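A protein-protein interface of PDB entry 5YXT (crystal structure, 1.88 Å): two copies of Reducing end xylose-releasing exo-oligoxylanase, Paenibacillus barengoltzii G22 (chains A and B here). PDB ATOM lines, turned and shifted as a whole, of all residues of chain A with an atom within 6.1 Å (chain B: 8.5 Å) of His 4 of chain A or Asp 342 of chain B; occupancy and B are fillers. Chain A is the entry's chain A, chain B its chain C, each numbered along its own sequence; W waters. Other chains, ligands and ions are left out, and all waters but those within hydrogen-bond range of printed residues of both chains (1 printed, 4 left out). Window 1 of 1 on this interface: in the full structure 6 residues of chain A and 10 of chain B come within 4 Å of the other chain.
His 4 of chain A touches just these residues of chain B: Ala 339, Asp 342, Leu 343 and Asn 346. Of chain A, only His 4 (2.9 Å) and Trp 273 (3.3 Å) come within 4 Å of Asp 342 of chain B. Printed residues of chain B within 4 Å of Arg 283 of chain A: Tyr 22 and Trp 345. Printed residues of chain A within 4 Å of Leu 343 of chain B: Met 1 (3.6 Å) and His 4 (3.4 Å). The nearest residue of chain B that does not touch His 4 of chain A is Lys 338 of chain B (5.0 Å). The nearest printed residue of chain A that does not touch Trp 345 of chain B is Pro 280 of chain A (6.4 Å).
The guanidinium group (NH1) of Arg 30 of chain B is in hydrogen-bond range of the backbone carbonyl oxygen (O) of Trp 345 of chain B (2.7 Å). N of Tyr 22 of chain B lies within hydrogen-bond range of O of Leu 17 of chain B (3.1 Å). The backbone carbonyl oxygen (O) of Leu 343 of chain B sits at hydrogen-bond distance from the side-chain hydroxyl (OG1) of Thr 347 of chain B, at 2.6 Å. OD1 of Asp 342 of chain B lies within hydrogen-bond range of OH of Tyr 22 of chain B, 2.5 Å away. The backbone NH of Met 1 of chain A is in hydrogen-bond range of the side-chain carboxylate of Glu 3 of chain A (2.5 Å). O of Glu 3 of chain A is in hydrogen-bond range of NE1 of Trp 273 of chain A, at 2.8 Å.
ND1 of His 4 of chain A sits at hydrogen-bond distance from OD2 of Asp 342 of chain B. The indole nitrogen of Trp 345 of chain B lies close to the guanidinium group of Arg 283 of chain A, at 2.5 Å. The backbone carbonyl oxygen (O) of Lys 296 of chain B sits close to the side-chain sulfur (SD) of Met 1 of chain A, 3.8 Å away.
No position is printed for both chains. Of the 12 pairs that touch across the chains among the printed residues, none has its exchanged pair printed and touching as well.
CG of Met 1 of chain A touches O of Ala 294 of chain B, at 3.6 Å. Met 1 of chain A touches Leu 343 of chain B. CB of Ala 339 of chain B touches O of His 4 of chain A, at 3.2 Å. CD1 of Leu 343 of chain B touches NE2 of His 4 of chain A (3.4 Å). CE1 of His 4 of chain A touches CB of Asn 346 of chain B, 3.9 Å away. CZ2 of Trp 273 of chain A touches OD2 of Asp 342 of chain B, 3.3 Å away. Tyr 20 of chain B touches Pro 280 of chain A (O to CD, 3.2 Å). Pro 280 of chain A touches Tyr 22 of chain B (CB to CE2, 3.6 Å). CD2 of Tyr 22 of chain B touches NH2 of Arg 283 of chain A, 3.9 Å away.
Of the 25 printed residues of chain B, 9 touch a printed residue of chain A. Printed residues of chain B that touch a printed residue of chain A: Tyr 20, Tyr 22, Ala 294, Lys 296, Ala 339, Asp 342, Leu 343, Trp 345 and Asn 346. Hydrophobic or aromatic side chains of chain B that line the printed part of chain A: Tyr 22, Ala 339, Leu 343 and Trp 345. Printed residues of chain A that touch a printed residue of chain B: Met 1, His 4, Trp 273, Pro 280 and Arg 283. Hydrophobic or aromatic side chains of chain A that line the printed part of chain B: Met 1, His 4, Trp 273 and Pro 280. Among the printed residues, no Asp or Glu carboxylate lies within 4 Å of a Lys or Arg side-chain nitrogen of the other chain.
Water W1 bridges NH1 of Arg 283 of chain A (2.6 Å) and OD1 of Asn 346 of chain B (2.9 Å).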
ATOM      1  N   MET A   1      -4.720 -22.444 -16.168  1.00  0.00           N
ATOM      2  CA  MET A   1      -4.072 -23.752 -16.194  1.00  0.00           C
ATOM      3  C   MET A   1      -3.961 -24.302 -17.615  1.00  0.00           C
ATOM      4  O   MET A   1      -2.922 -24.865 -18.002  1.00  0.00           O
ATOM      5  CB  MET A   1      -4.841 -24.746 -15.318  1.00  0.00           C
ATOM      6  CG  MET A   1      -4.024 -25.973 -14.930  1.00  0.00           C
ATOM      7  SD  MET A   1      -2.339 -25.525 -14.433  1.00  0.00           S
ATOM      8  CE  MET A   1      -1.360 -26.475 -15.594  1.00  0.00           C
ATOM      9  N   LYS A   2      -5.046 -24.145 -18.380  1.00  0.00           N
ATOM     10  CA  LYS A   2      -5.093 -24.639 -19.751  1.00  0.00           C
ATOM     11  C   LYS A   2      -4.081 -23.944 -20.652  1.00  0.00           C
ATOM     12  O   LYS A   2      -3.803 -24.443 -21.747  1.00  0.00           O
ATOM     13  CB  LYS A   2      -6.503 -24.467 -20.320  1.00  0.00           C
ATOM     14  N   GLU A   3      -3.539 -22.806 -20.212  1.00  0.00           N
ATOM     15  CA  GLU A   3      -2.477 -22.118 -20.942  1.00  0.00           C
ATOM     16  C   GLU A   3      -1.209 -22.961 -21.032  1.00  0.00           C
ATOM     17  O   GLU A   3      -0.393 -22.760 -21.941  1.00  0.00           O
ATOM     18  CB  GLU A   3      -2.151 -20.783 -20.263  1.00  0.00           C
ATOM     19  CG  GLU A   3      -3.334 -19.835 -20.074  1.00  0.00           C
ATOM     20  CD  GLU A   3      -4.163 -20.147 -18.834  1.00  0.00           C
ATOM     21  OE1 GLU A   3      -5.232 -19.517 -18.655  1.00  0.00           O
ATOM     22  OE2 GLU A   3      -3.754 -21.026 -18.039  1.00  0.00           O
ATOM     23  N   HIS A   4      -1.016 -23.891 -20.095  1.00  0.00           N
ATOM     24  CA  HIS A   4       0.219 -24.662 -19.988  1.00  0.00           C
ATOM     25  C   HIS A   4       0.047 -26.127 -20.352  1.00  0.00           C
ATOM     26  O   HIS A   4       1.018 -26.888 -20.303  1.00  0.00           O
ATOM     27  CB  HIS A   4       0.761 -24.526 -18.562  1.00  0.00           C
ATOM     28  CG  HIS A   4       0.629 -23.137 -18.032  1.00  0.00           C
ATOM     29  ND1 HIS A   4       1.440 -22.106 -18.448  1.00  0.00           N
ATOM     30  CD2 HIS A   4      -0.273 -22.589 -17.186  1.00  0.00           C
ATOM     31  CE1 HIS A   4       1.074 -20.989 -17.847  1.00  0.00           C
ATOM     32  NE2 HIS A   4       0.043 -21.258 -17.066  1.00  0.00           N
ATOM     33  N   GLN A   5      -1.155 -26.533 -20.725  1.00  0.00           N
ATOM     34  CA  GLN A   5      -1.490 -27.925 -20.958  1.00  0.00           C
ATOM     35  C   GLN A   5      -2.033 -28.040 -22.369  1.00  0.00           C
ATOM     36  O   GLN A   5      -2.880 -27.236 -22.771  1.00  0.00           O
ATOM     37  CB  GLN A   5      -2.524 -28.418 -19.944  1.00  0.00           C
ATOM     38  N   GLY A   6      -1.517 -29.002 -23.126  1.00  0.00           N
ATOM     39  CA  GLY A   6      -2.001 -29.197 -24.481  1.00  0.00           C
ATOM     40  C   GLY A   6      -3.424 -29.720 -24.463  1.00  0.00           C
ATOM     41  O   GLY A   6      -3.740 -30.681 -23.750  1.00  0.00           O
ATOM     42  N   ARG A  14      -9.139 -23.455 -24.135  1.00  0.00           N
ATOM     43  CA  ARG A  14      -9.300 -22.083 -23.679  1.00  0.00           C
ATOM     44  C   ARG A  14     -10.234 -21.314 -24.603  1.00  0.00           C
ATOM     45  O   ARG A  14     -10.122 -21.400 -25.828  1.00  0.00           O
ATOM     46  CB  ARG A  14      -7.940 -21.392 -23.630  1.00  0.00           C
ATOM     47  CG  ARG A  14      -7.121 -21.726 -22.406  1.00  0.00           C
ATOM     48  CD  ARG A  14      -5.804 -20.959 -22.406  1.00  0.00           C
ATOM     49  NE  ARG A  14      -4.907 -21.482 -23.428  1.00  0.00           N
ATOM     50  CZ  ARG A  14      -3.880 -20.816 -23.943  1.00  0.00           C
ATOM     51  NH1 ARG A  14      -3.604 -19.585 -23.526  1.00  0.00           N
ATOM     52  NH2 ARG A  14      -3.127 -21.393 -24.878  1.00  0.00           N
ATOM     53  N   TRP A 273       0.797 -24.480 -29.737  1.00  0.00           N
ATOM     54  CA  TRP A 273       0.969 -24.323 -28.293  1.00  0.00           C
ATOM     55  C   TRP A 273      -0.302 -24.699 -27.545  1.00  0.00           C
ATOM     56  O   TRP A 273      -0.249 -25.427 -26.544  1.00  0.00           O
ATOM     57  CB  TRP A 273       1.385 -22.898 -27.924  1.00  0.00           C
ATOM     58  CG  TRP A 273       1.573 -22.842 -26.444  1.00  0.00           C
ATOM     59  CD1 TRP A 273       0.692 -22.357 -25.516  1.00  0.00           C
ATOM     60  CD2 TRP A 273       2.666 -23.391 -25.711  1.00  0.00           C
ATOM     61  NE1 TRP A 273       1.192 -22.545 -24.248  1.00  0.00           N
ATOM     62  CE2 TRP A 273       2.403 -23.178 -24.341  1.00  0.00           C
ATOM     63  CE3 TRP A 273       3.844 -24.043 -26.079  1.00  0.00           C
ATOM     64  CZ2 TRP A 273       3.281 -23.586 -23.340  1.00  0.00           C
ATOM     65  CZ3 TRP A 273       4.722 -24.457 -25.078  1.00  0.00           C
ATOM     66  CH2 TRP A 273       4.433 -24.222 -23.726  1.00  0.00           C
ATOM     67  N   ALA A 277       1.270 -27.725 -26.377  1.00  0.00           N
ATOM     68  CA  ALA A 277       2.144 -27.070 -25.404  1.00  0.00           C
ATOM     69  C   ALA A 277       3.503 -27.769 -25.332  1.00  0.00           C
ATOM     70  O   ALA A 277       4.039 -28.049 -24.257  1.00  0.00           O
ATOM     71  CB  ALA A 277       1.471 -27.009 -24.031  1.00  0.00           C
ATOM     72  N   PRO A 280       8.356 -24.667 -25.591  1.00  0.00           N
ATOM     73  CA  PRO A 280       8.279 -23.327 -24.984  1.00  0.00           C
ATOM     74  C   PRO A 280       8.849 -22.216 -25.861  1.00  0.00           C
ATOM     75  O   PRO A 280       8.456 -21.051 -25.711  1.00  0.00           O
ATOM     76  CB  PRO A 280       9.084 -23.492 -23.687  1.00  0.00           C
ATOM     77  CG  PRO A 280       9.022 -24.989 -23.382  1.00  0.00           C
ATOM     78  CD  PRO A 280       8.991 -25.667 -24.712  1.00  0.00           C
ATOM     79  N   ARG A 283       6.420 -19.645 -27.498  1.00  0.00           N
ATOM     80  CA  ARG A 283       5.905 -18.455 -26.843  1.00  0.00           C
ATOM     81  C   ARG A 283       6.898 -17.293 -26.960  1.00  0.00           C
ATOM     82  O   ARG A 283       6.490 -16.134 -27.114  1.00  0.00           O
ATOM     83  CB  ARG A 283       5.556 -18.794 -25.398  1.00  0.00           C
ATOM     84  CG  ARG A 283       6.691 -18.515 -24.504  1.00  0.00           C
ATOM     85  CD  ARG A 283       6.821 -19.549 -23.309  1.00  0.00           C
ATOM     86  NE  ARG A 283       8.143 -19.500 -22.657  1.00  0.00           N
ATOM     87  CZ  ARG A 283       8.656 -18.467 -21.967  1.00  0.00           C
ATOM     88  NH1 ARG A 283       8.002 -17.349 -21.787  1.00  0.00           N
ATOM     89  NH2 ARG A 283       9.882 -18.584 -21.462  1.00  0.00           N
ATOM     90  N   ASP A 333       1.156 -14.012 -23.430  1.00  0.00           N
ATOM     91  CA  ASP A 333       0.402 -13.447 -22.315  1.00  0.00           C
ATOM     92  C   ASP A 333       1.025 -12.112 -21.944  1.00  0.00           C
ATOM     93  O   ASP A 333       2.215 -11.883 -22.176  1.00  0.00           O
ATOM     94  CB  ASP A 333       0.371 -14.380 -21.097  1.00  0.00           C
ATOM     95  CG  ASP A 333      -0.866 -15.277 -21.074  1.00  0.00           C
ATOM     96  OD1 ASP A 333      -1.971 -14.773 -20.774  1.00  0.00           O
ATOM     97  OD2 ASP A 333      -0.734 -16.492 -21.353  1.00  0.00           O
ATOM     98  N   LEU B  17      14.930 -27.408 -16.986  1.00  0.00           N
ATOM     99  CA  LEU B  17      14.363 -26.311 -17.772  1.00  0.00           C
ATOM    100  C   LEU B  17      14.982 -26.263 -19.166  1.00  0.00           C
ATOM    101  O   LEU B  17      14.272 -26.110 -20.166  1.00  0.00           O
ATOM    102  CB  LEU B  17      14.573 -24.985 -17.048  1.00  0.00           C
ATOM    103  CG  LEU B  17      13.732 -24.796 -15.783  1.00  0.00           C
ATOM    104  CD1 LEU B  17      14.244 -23.657 -14.905  1.00  0.00           C
ATOM    105  CD2 LEU B  17      12.290 -24.577 -16.160  1.00  0.00           C
ATOM    106  N   TYR B  20      13.743 -29.022 -21.276  1.00  0.00           N
ATOM    107  CA  TYR B  20      12.373 -28.753 -21.663  1.00  0.00           C
ATOM    108  C   TYR B  20      12.254 -27.656 -22.714  1.00  0.00           C
ATOM    109  O   TYR B  20      11.158 -27.456 -23.242  1.00  0.00           O
ATOM    110  CB  TYR B  20      11.563 -28.364 -20.423  1.00  0.00           C
ATOM    111  CG  TYR B  20      11.069 -29.532 -19.589  1.00  0.00           C
ATOM    112  CD1 TYR B  20      11.594 -30.817 -19.755  1.00  0.00           C
ATOM    113  CD2 TYR B  20      10.083 -29.345 -18.623  1.00  0.00           C
ATOM    114  CE1 TYR B  20      11.131 -31.884 -18.988  1.00  0.00           C
ATOM    115  CE2 TYR B  20       9.616 -30.403 -17.851  1.00  0.00           C
ATOM    116  CZ  TYR B  20      10.137 -31.659 -18.033  1.00  0.00           C
ATOM    117  OH  TYR B  20       9.656 -32.685 -17.253  1.00  0.00           O
ATOM    118  N   GLY B  21      13.334 -26.936 -23.019  1.00  0.00           N
ATOM    119  CA  GLY B  21      13.329 -25.986 -24.116  1.00  0.00           C
ATOM    120  C   GLY B  21      13.325 -24.529 -23.714  1.00  0.00           C
ATOM    121  O   GLY B  21      13.213 -23.665 -24.594  1.00  0.00           O
ATOM    122  N   TYR B  22      13.415 -24.219 -22.423  1.00  0.00           N
ATOM    123  CA  TYR B  22      13.633 -22.843 -22.011  1.00  0.00           C
ATOM    124  C   TYR B  22      15.100 -22.494 -22.267  1.00  0.00           C
ATOM    125  O   TYR B  22      15.981 -23.359 -22.246  1.00  0.00           O
ATOM    126  CB  TYR B  22      13.218 -22.657 -20.534  1.00  0.00           C
ATOM    127  CG  TYR B  22      11.783 -23.109 -20.291  1.00  0.00           C
ATOM    128  CD1 TYR B  22      11.499 -24.435 -19.966  1.00  0.00           C
ATOM    129  CD2 TYR B  22      10.710 -22.217 -20.428  1.00  0.00           C
ATOM    130  CE1 TYR B  22      10.198 -24.866 -19.772  1.00  0.00           C
ATOM    131  CE2 TYR B  22       9.397 -22.637 -20.240  1.00  0.00           C
ATOM    132  CZ  TYR B  22       9.146 -23.961 -19.911  1.00  0.00           C
ATOM    133  OH  TYR B  22       7.861 -24.405 -19.720  1.00  0.00           O
ATOM    134  N   ARG B  30      16.555 -15.758 -14.789  1.00  0.00           N
ATOM    135  CA  ARG B  30      15.459 -15.978 -13.850  1.00  0.00           C
ATOM    136  C   ARG B  30      15.979 -16.326 -12.461  1.00  0.00           C
ATOM    137  O   ARG B  30      15.490 -15.800 -11.454  1.00  0.00           O
ATOM    138  CB  ARG B  30      14.541 -17.080 -14.368  1.00  0.00           C
ATOM    139  CG  ARG B  30      13.231 -17.203 -13.603  1.00  0.00           C
ATOM    140  CD  ARG B  30      12.378 -15.941 -13.709  1.00  0.00           C
ATOM    141  NE  ARG B  30      11.688 -15.876 -14.991  1.00  0.00           N
ATOM    142  CZ  ARG B  30      10.663 -16.648 -15.333  1.00  0.00           C
ATOM    143  NH1 ARG B  30      10.192 -17.544 -14.478  1.00  0.00           N
ATOM    144  NH2 ARG B  30      10.108 -16.519 -16.535  1.00  0.00           N
ATOM    145  N   ALA B 294      -3.495 -31.597 -12.327  1.00  0.00           N
ATOM    146  CA  ALA B 294      -3.575 -31.229 -13.738  1.00  0.00           C
ATOM    147  C   ALA B 294      -4.879 -30.505 -14.059  1.00  0.00           C
ATOM    148  O   ALA B 294      -4.876 -29.518 -14.801  1.00  0.00           O
ATOM    149  CB  ALA B 294      -3.427 -32.473 -14.612  1.00  0.00           C
ATOM    150  N   LYS B 296      -6.633 -28.476 -12.297  1.00  0.00           N
ATOM    151  CA  LYS B 296      -6.896 -27.535 -11.220  1.00  0.00           C
ATOM    152  C   LYS B 296      -6.213 -26.202 -11.481  1.00  0.00           C
ATOM    153  O   LYS B 296      -5.062 -26.153 -11.925  1.00  0.00           O
ATOM    154  CB  LYS B 296      -6.446 -28.105  -9.872  1.00  0.00           C
ATOM    155  CG  LYS B 296      -7.336 -29.229  -9.385  1.00  0.00           C
ATOM    156  CD  LYS B 296      -7.134 -29.487  -7.909  1.00  0.00           C
ATOM    157  CE  LYS B 296      -8.188 -30.434  -7.391  1.00  0.00           C
ATOM    158  NZ  LYS B 296      -8.291 -31.662  -8.208  1.00  0.00           N
ATOM    159  N   PRO B 298      -4.536 -22.846 -10.044  1.00  0.00           N
ATOM    160  CA  PRO B 298      -3.871 -22.378  -8.819  1.00  0.00           C
ATOM    161  C   PRO B 298      -4.679 -21.353  -8.047  1.00  0.00           C
ATOM    162  O   PRO B 298      -4.684 -21.384  -6.809  1.00  0.00           O
ATOM    163  CB  PRO B 298      -2.557 -21.789  -9.353  1.00  0.00           C
ATOM    164  CG  PRO B 298      -2.352 -22.440 -10.685  1.00  0.00           C
ATOM    165  CD  PRO B 298      -3.707 -22.658 -11.247  1.00  0.00           C
ATOM    166  N   LEU B 322       2.328 -24.891  -6.370  1.00  0.00           N
ATOM    167  CA  LEU B 322       2.689 -25.117  -7.768  1.00  0.00           C
ATOM    168  C   LEU B 322       4.201 -25.227  -7.947  1.00  0.00           C
ATOM    169  O   LEU B 322       4.660 -25.913  -8.870  1.00  0.00           O
ATOM    170  CB  LEU B 322       2.100 -24.029  -8.667  1.00  0.00           C
ATOM    171  CG  LEU B 322       2.682 -22.616  -8.617  1.00  0.00           C
ATOM    172  CD1 LEU B 322       3.849 -22.489  -9.577  1.00  0.00           C
ATOM    173  CD2 LEU B 322       1.608 -21.594  -8.937  1.00  0.00           C
ATOM    174  N   ALA B 326       6.099 -28.502  -9.616  1.00  0.00           N
ATOM    175  CA  ALA B 326       7.073 -28.347 -10.689  1.00  0.00           C
ATOM    176  C   ALA B 326       8.390 -29.034 -10.346  1.00  0.00           C
ATOM    177  O   ALA B 326       8.980 -29.715 -11.191  1.00  0.00           O
ATOM    178  CB  ALA B 326       7.295 -26.861 -10.975  1.00  0.00           C
ATOM    179  N   SER B 329       8.783 -32.689 -11.072  1.00  0.00           N
ATOM    180  CA  SER B 329       9.014 -33.160 -12.438  1.00  0.00           C
ATOM    181  C   SER B 329      10.394 -33.783 -12.627  1.00  0.00           C
ATOM    182  O   SER B 329      10.613 -34.483 -13.621  1.00  0.00           O
ATOM    183  CB  SER B 329       8.820 -32.004 -13.422  1.00  0.00           C
ATOM    184  OG  SER B 329       7.436 -31.700 -13.580  1.00  0.00           O
ATOM    185  N   PRO B 335       3.617 -35.158 -20.792  1.00  0.00           N
ATOM    186  CA  PRO B 335       3.052 -33.802 -20.918  1.00  0.00           C
ATOM    187  C   PRO B 335       2.638 -33.172 -19.599  1.00  0.00           C
ATOM    188  O   PRO B 335       2.713 -31.945 -19.478  1.00  0.00           O
ATOM    189  CB  PRO B 335       1.846 -34.012 -21.844  1.00  0.00           C
ATOM    190  CG  PRO B 335       1.503 -35.469 -21.693  1.00  0.00           C
ATOM    191  CD  PRO B 335       2.819 -36.160 -21.517  1.00  0.00           C
ATOM    192  N   GLN B 336       2.188 -33.950 -18.608  1.00  0.00           N
ATOM    193  CA  GLN B 336       1.797 -33.321 -17.352  1.00  0.00           C
ATOM    194  C   GLN B 336       3.010 -32.800 -16.594  1.00  0.00           C
ATOM    195  O   GLN B 336       2.912 -31.782 -15.904  1.00  0.00           O
ATOM    196  CB  GLN B 336       0.987 -34.294 -16.484  1.00  0.00           C
ATOM    197  CG  GLN B 336      -0.487 -34.430 -16.907  1.00  0.00           C
ATOM    198  CD  GLN B 336      -1.265 -35.441 -16.078  1.00  0.00           C
ATOM    199  OE1 GLN B 336      -0.687 -36.322 -15.433  1.00  0.00           O
ATOM    200  NE2 GLN B 336      -2.589 -35.325 -16.101  1.00  0.00           N
ATOM    201  N   ALA B 337       4.153 -33.479 -16.711  1.00  0.00           N
ATOM    202  CA  ALA B 337       5.374 -32.988 -16.078  1.00  0.00           C
ATOM    203  C   ALA B 337       5.830 -31.686 -16.711  1.00  0.00           C
ATOM    204  O   ALA B 337       6.244 -30.755 -16.011  1.00  0.00           O
ATOM    205  CB  ALA B 337       6.476 -34.042 -16.179  1.00  0.00           C
ATOM    206  N   LYS B 338       5.758 -31.601 -18.039  1.00  0.00           N
ATOM    207  CA  LYS B 338       6.108 -30.360 -18.715  1.00  0.00           C
ATOM    208  C   LYS B 338       5.112 -29.251 -18.406  1.00  0.00           C
ATOM    209  O   LYS B 338       5.501 -28.081 -18.318  1.00  0.00           O
ATOM    210  CB  LYS B 338       6.194 -30.596 -20.221  1.00  0.00           C
ATOM    211  N   ALA B 339       3.835 -29.592 -18.231  1.00  0.00           N
ATOM    212  CA  ALA B 339       2.844 -28.571 -17.918  1.00  0.00           C
ATOM    213  C   ALA B 339       3.062 -27.989 -16.521  1.00  0.00           C
ATOM    214  O   ALA B 339       2.970 -26.769 -16.333  1.00  0.00           O
ATOM    215  CB  ALA B 339       1.436 -29.145 -18.056  1.00  0.00           C
ATOM    216  N   CYS B 340       3.354 -28.841 -15.532  1.00  0.00           N
ATOM    217  CA  CYS B 340       3.650 -28.338 -14.190  1.00  0.00           C
ATOM    218  C   CYS B 340       4.824 -27.368 -14.212  1.00  0.00           C
ATOM    219  O   CYS B 340       4.812 -26.346 -13.517  1.00  0.00           O
ATOM    220  CB  CYS B 340       3.937 -29.499 -13.235  1.00  0.00           C
ATOM    221  SG  CYS B 340       2.441 -30.421 -12.708  1.00  0.00           S
ATOM    222  N   VAL B 341       5.832 -27.655 -15.032  1.00  0.00           N
ATOM    223  CA  VAL B 341       7.005 -26.794 -15.092  1.00  0.00           C
ATOM    224  C   VAL B 341       6.676 -25.492 -15.815  1.00  0.00           C
ATOM    225  O   VAL B 341       7.139 -24.421 -15.411  1.00  0.00           O
ATOM    226  CB  VAL B 341       8.179 -27.547 -15.748  1.00  0.00           C
ATOM    227  CG1 VAL B 341       9.343 -26.614 -16.028  1.00  0.00           C
ATOM    228  CG2 VAL B 341       8.634 -28.669 -14.847  1.00  0.00           C
ATOM    229  N   ASP B 342       5.862 -25.557 -16.885  1.00  0.00           N
ATOM    230  CA  ASP B 342       5.502 -24.336 -17.610  1.00  0.00           C
ATOM    231  C   ASP B 342       4.651 -23.403 -16.761  1.00  0.00           C
ATOM    232  O   ASP B 342       4.801 -22.175 -16.840  1.00  0.00           O
ATOM    233  CB  ASP B 342       4.756 -24.643 -18.907  1.00  0.00           C
ATOM    234  CG  ASP B 342       4.736 -23.447 -19.840  1.00  0.00           C
ATOM    235  OD1 ASP B 342       5.842 -23.027 -20.257  1.00  0.00           O
ATOM    236  OD2 ASP B 342       3.640 -22.902 -20.128  1.00  0.00           O
ATOM    237  N   LEU B 343       3.726 -23.951 -15.979  1.00  0.00           N
ATOM    238  CA  LEU B 343       2.988 -23.105 -15.051  1.00  0.00           C
ATOM    239  C   LEU B 343       3.943 -22.396 -14.097  1.00  0.00           C
ATOM    240  O   LEU B 343       3.874 -21.177 -13.920  1.00  0.00           O
ATOM    241  CB  LEU B 343       1.963 -23.937 -14.281  1.00  0.00           C
ATOM    242  CG  LEU B 343       1.135 -23.232 -13.209  1.00  0.00           C
ATOM    243  CD1 LEU B 343       0.184 -22.220 -13.812  1.00  0.00           C
ATOM    244  CD2 LEU B 343       0.359 -24.297 -12.417  1.00  0.00           C
ATOM    245  N   PHE B 344       4.875 -23.143 -13.507  1.00  0.00           N
ATOM    246  CA  PHE B 344       5.833 -22.530 -12.591  1.00  0.00           C
ATOM    247  C   PHE B 344       6.690 -21.485 -13.294  1.00  0.00           C
ATOM    248  O   PHE B 344       6.941 -20.404 -12.744  1.00  0.00           O
ATOM    249  CB  PHE B 344       6.716 -23.611 -11.968  1.00  0.00           C
ATOM    250  CG  PHE B 344       7.893 -23.063 -11.221  1.00  0.00           C
ATOM    251  CD1 PHE B 344       7.710 -22.348 -10.042  1.00  0.00           C
ATOM    252  CD2 PHE B 344       9.183 -23.256 -11.702  1.00  0.00           C
ATOM    253  CE1 PHE B 344       8.815 -21.828  -9.342  1.00  0.00           C
ATOM    254  CE2 PHE B 344      10.292 -22.742 -11.011  1.00  0.00           C
ATOM    255  CZ  PHE B 344      10.104 -22.026  -9.840  1.00  0.00           C
ATOM    256  N   TRP B 345       7.163 -21.794 -14.507  1.00  0.00           N
ATOM    257  CA  TRP B 345       7.991 -20.835 -15.232  1.00  0.00           C
ATOM    258  C   TRP B 345       7.246 -19.521 -15.434  1.00  0.00           C
ATOM    259  O   TRP B 345       7.849 -18.439 -15.376  1.00  0.00           O
ATOM    260  CB  TRP B 345       8.436 -21.422 -16.580  1.00  0.00           C
ATOM    261  CG  TRP B 345       9.253 -20.471 -17.412  1.00  0.00           C
ATOM    262  CD1 TRP B 345       8.821 -19.741 -18.485  1.00  0.00           C
ATOM    263  CD2 TRP B 345      10.639 -20.151 -17.244  1.00  0.00           C
ATOM    264  NE1 TRP B 345       9.846 -18.976 -18.978  1.00  0.00           N
ATOM    265  CE2 TRP B 345      10.974 -19.213 -18.241  1.00  0.00           C
ATOM    266  CE3 TRP B 345      11.626 -20.560 -16.344  1.00  0.00           C
ATOM    267  CZ2 TRP B 345      12.248 -18.675 -18.359  1.00  0.00           C
ATOM    268  CZ3 TRP B 345      12.895 -20.022 -16.461  1.00  0.00           C
ATOM    269  CH2 TRP B 345      13.195 -19.094 -17.465  1.00  0.00           C
ATOM    270  N   ASN B 346       5.934 -19.591 -15.647  1.00  0.00           N
ATOM    271  CA  ASN B 346       5.131 -18.400 -15.899  1.00  0.00           C
ATOM    272  C   ASN B 346       4.485 -17.833 -14.635  1.00  0.00           C
ATOM    273  O   ASN B 346       3.515 -17.074 -14.733  1.00  0.00           O
ATOM    274  CB  ASN B 346       4.085 -18.699 -16.972  1.00  0.00           C
ATOM    275  CG  ASN B 346       4.720 -18.868 -18.338  1.00  0.00           C
ATOM    276  OD1 ASN B 346       5.068 -17.889 -18.989  1.00  0.00           O
ATOM    277  ND2 ASN B 346       4.913 -20.114 -18.760  1.00  0.00           N
ATOM    278  N   THR B 347       5.028 -18.155 -13.461  1.00  0.00           N
ATOM    279  CA  THR B 347       4.493 -17.688 -12.183  1.00  0.00           C
ATOM    280  C   THR B 347       5.538 -16.807 -11.525  1.00  0.00           C
ATOM    281  O   THR B 347       6.669 -17.271 -11.312  1.00  0.00           O
ATOM    282  CB  THR B 347       4.140 -18.859 -11.271  1.00  0.00           C
ATOM    283  OG1 THR B 347       3.136 -19.659 -11.893  1.00  0.00           O
ATOM    284  CG2 THR B 347       3.600 -18.360  -9.903  1.00  0.00           C
ATOM    285  N   LEU B 369      15.329 -27.204 -10.627  1.00  0.00           N
ATOM    286  CA  LEU B 369      14.957 -27.383 -12.027  1.00  0.00           C
ATOM    287  C   LEU B 369      15.984 -26.806 -12.988  1.00  0.00           C
ATOM    288  O   LEU B 369      15.909 -27.083 -14.189  1.00  0.00           O
ATOM    289  CB  LEU B 369      13.595 -26.740 -12.306  1.00  0.00           C
ATOM    290  CG  LEU B 369      12.404 -27.447 -11.661  1.00  0.00           C
ATOM    291  CD1 LEU B 369      11.153 -26.571 -11.738  1.00  0.00           C
ATOM    292  CD2 LEU B 369      12.176 -28.805 -12.312  1.00  0.00           C
HETATM  293  O   HOH W   1       6.772 -15.797 -20.036  1.00  0.00           O
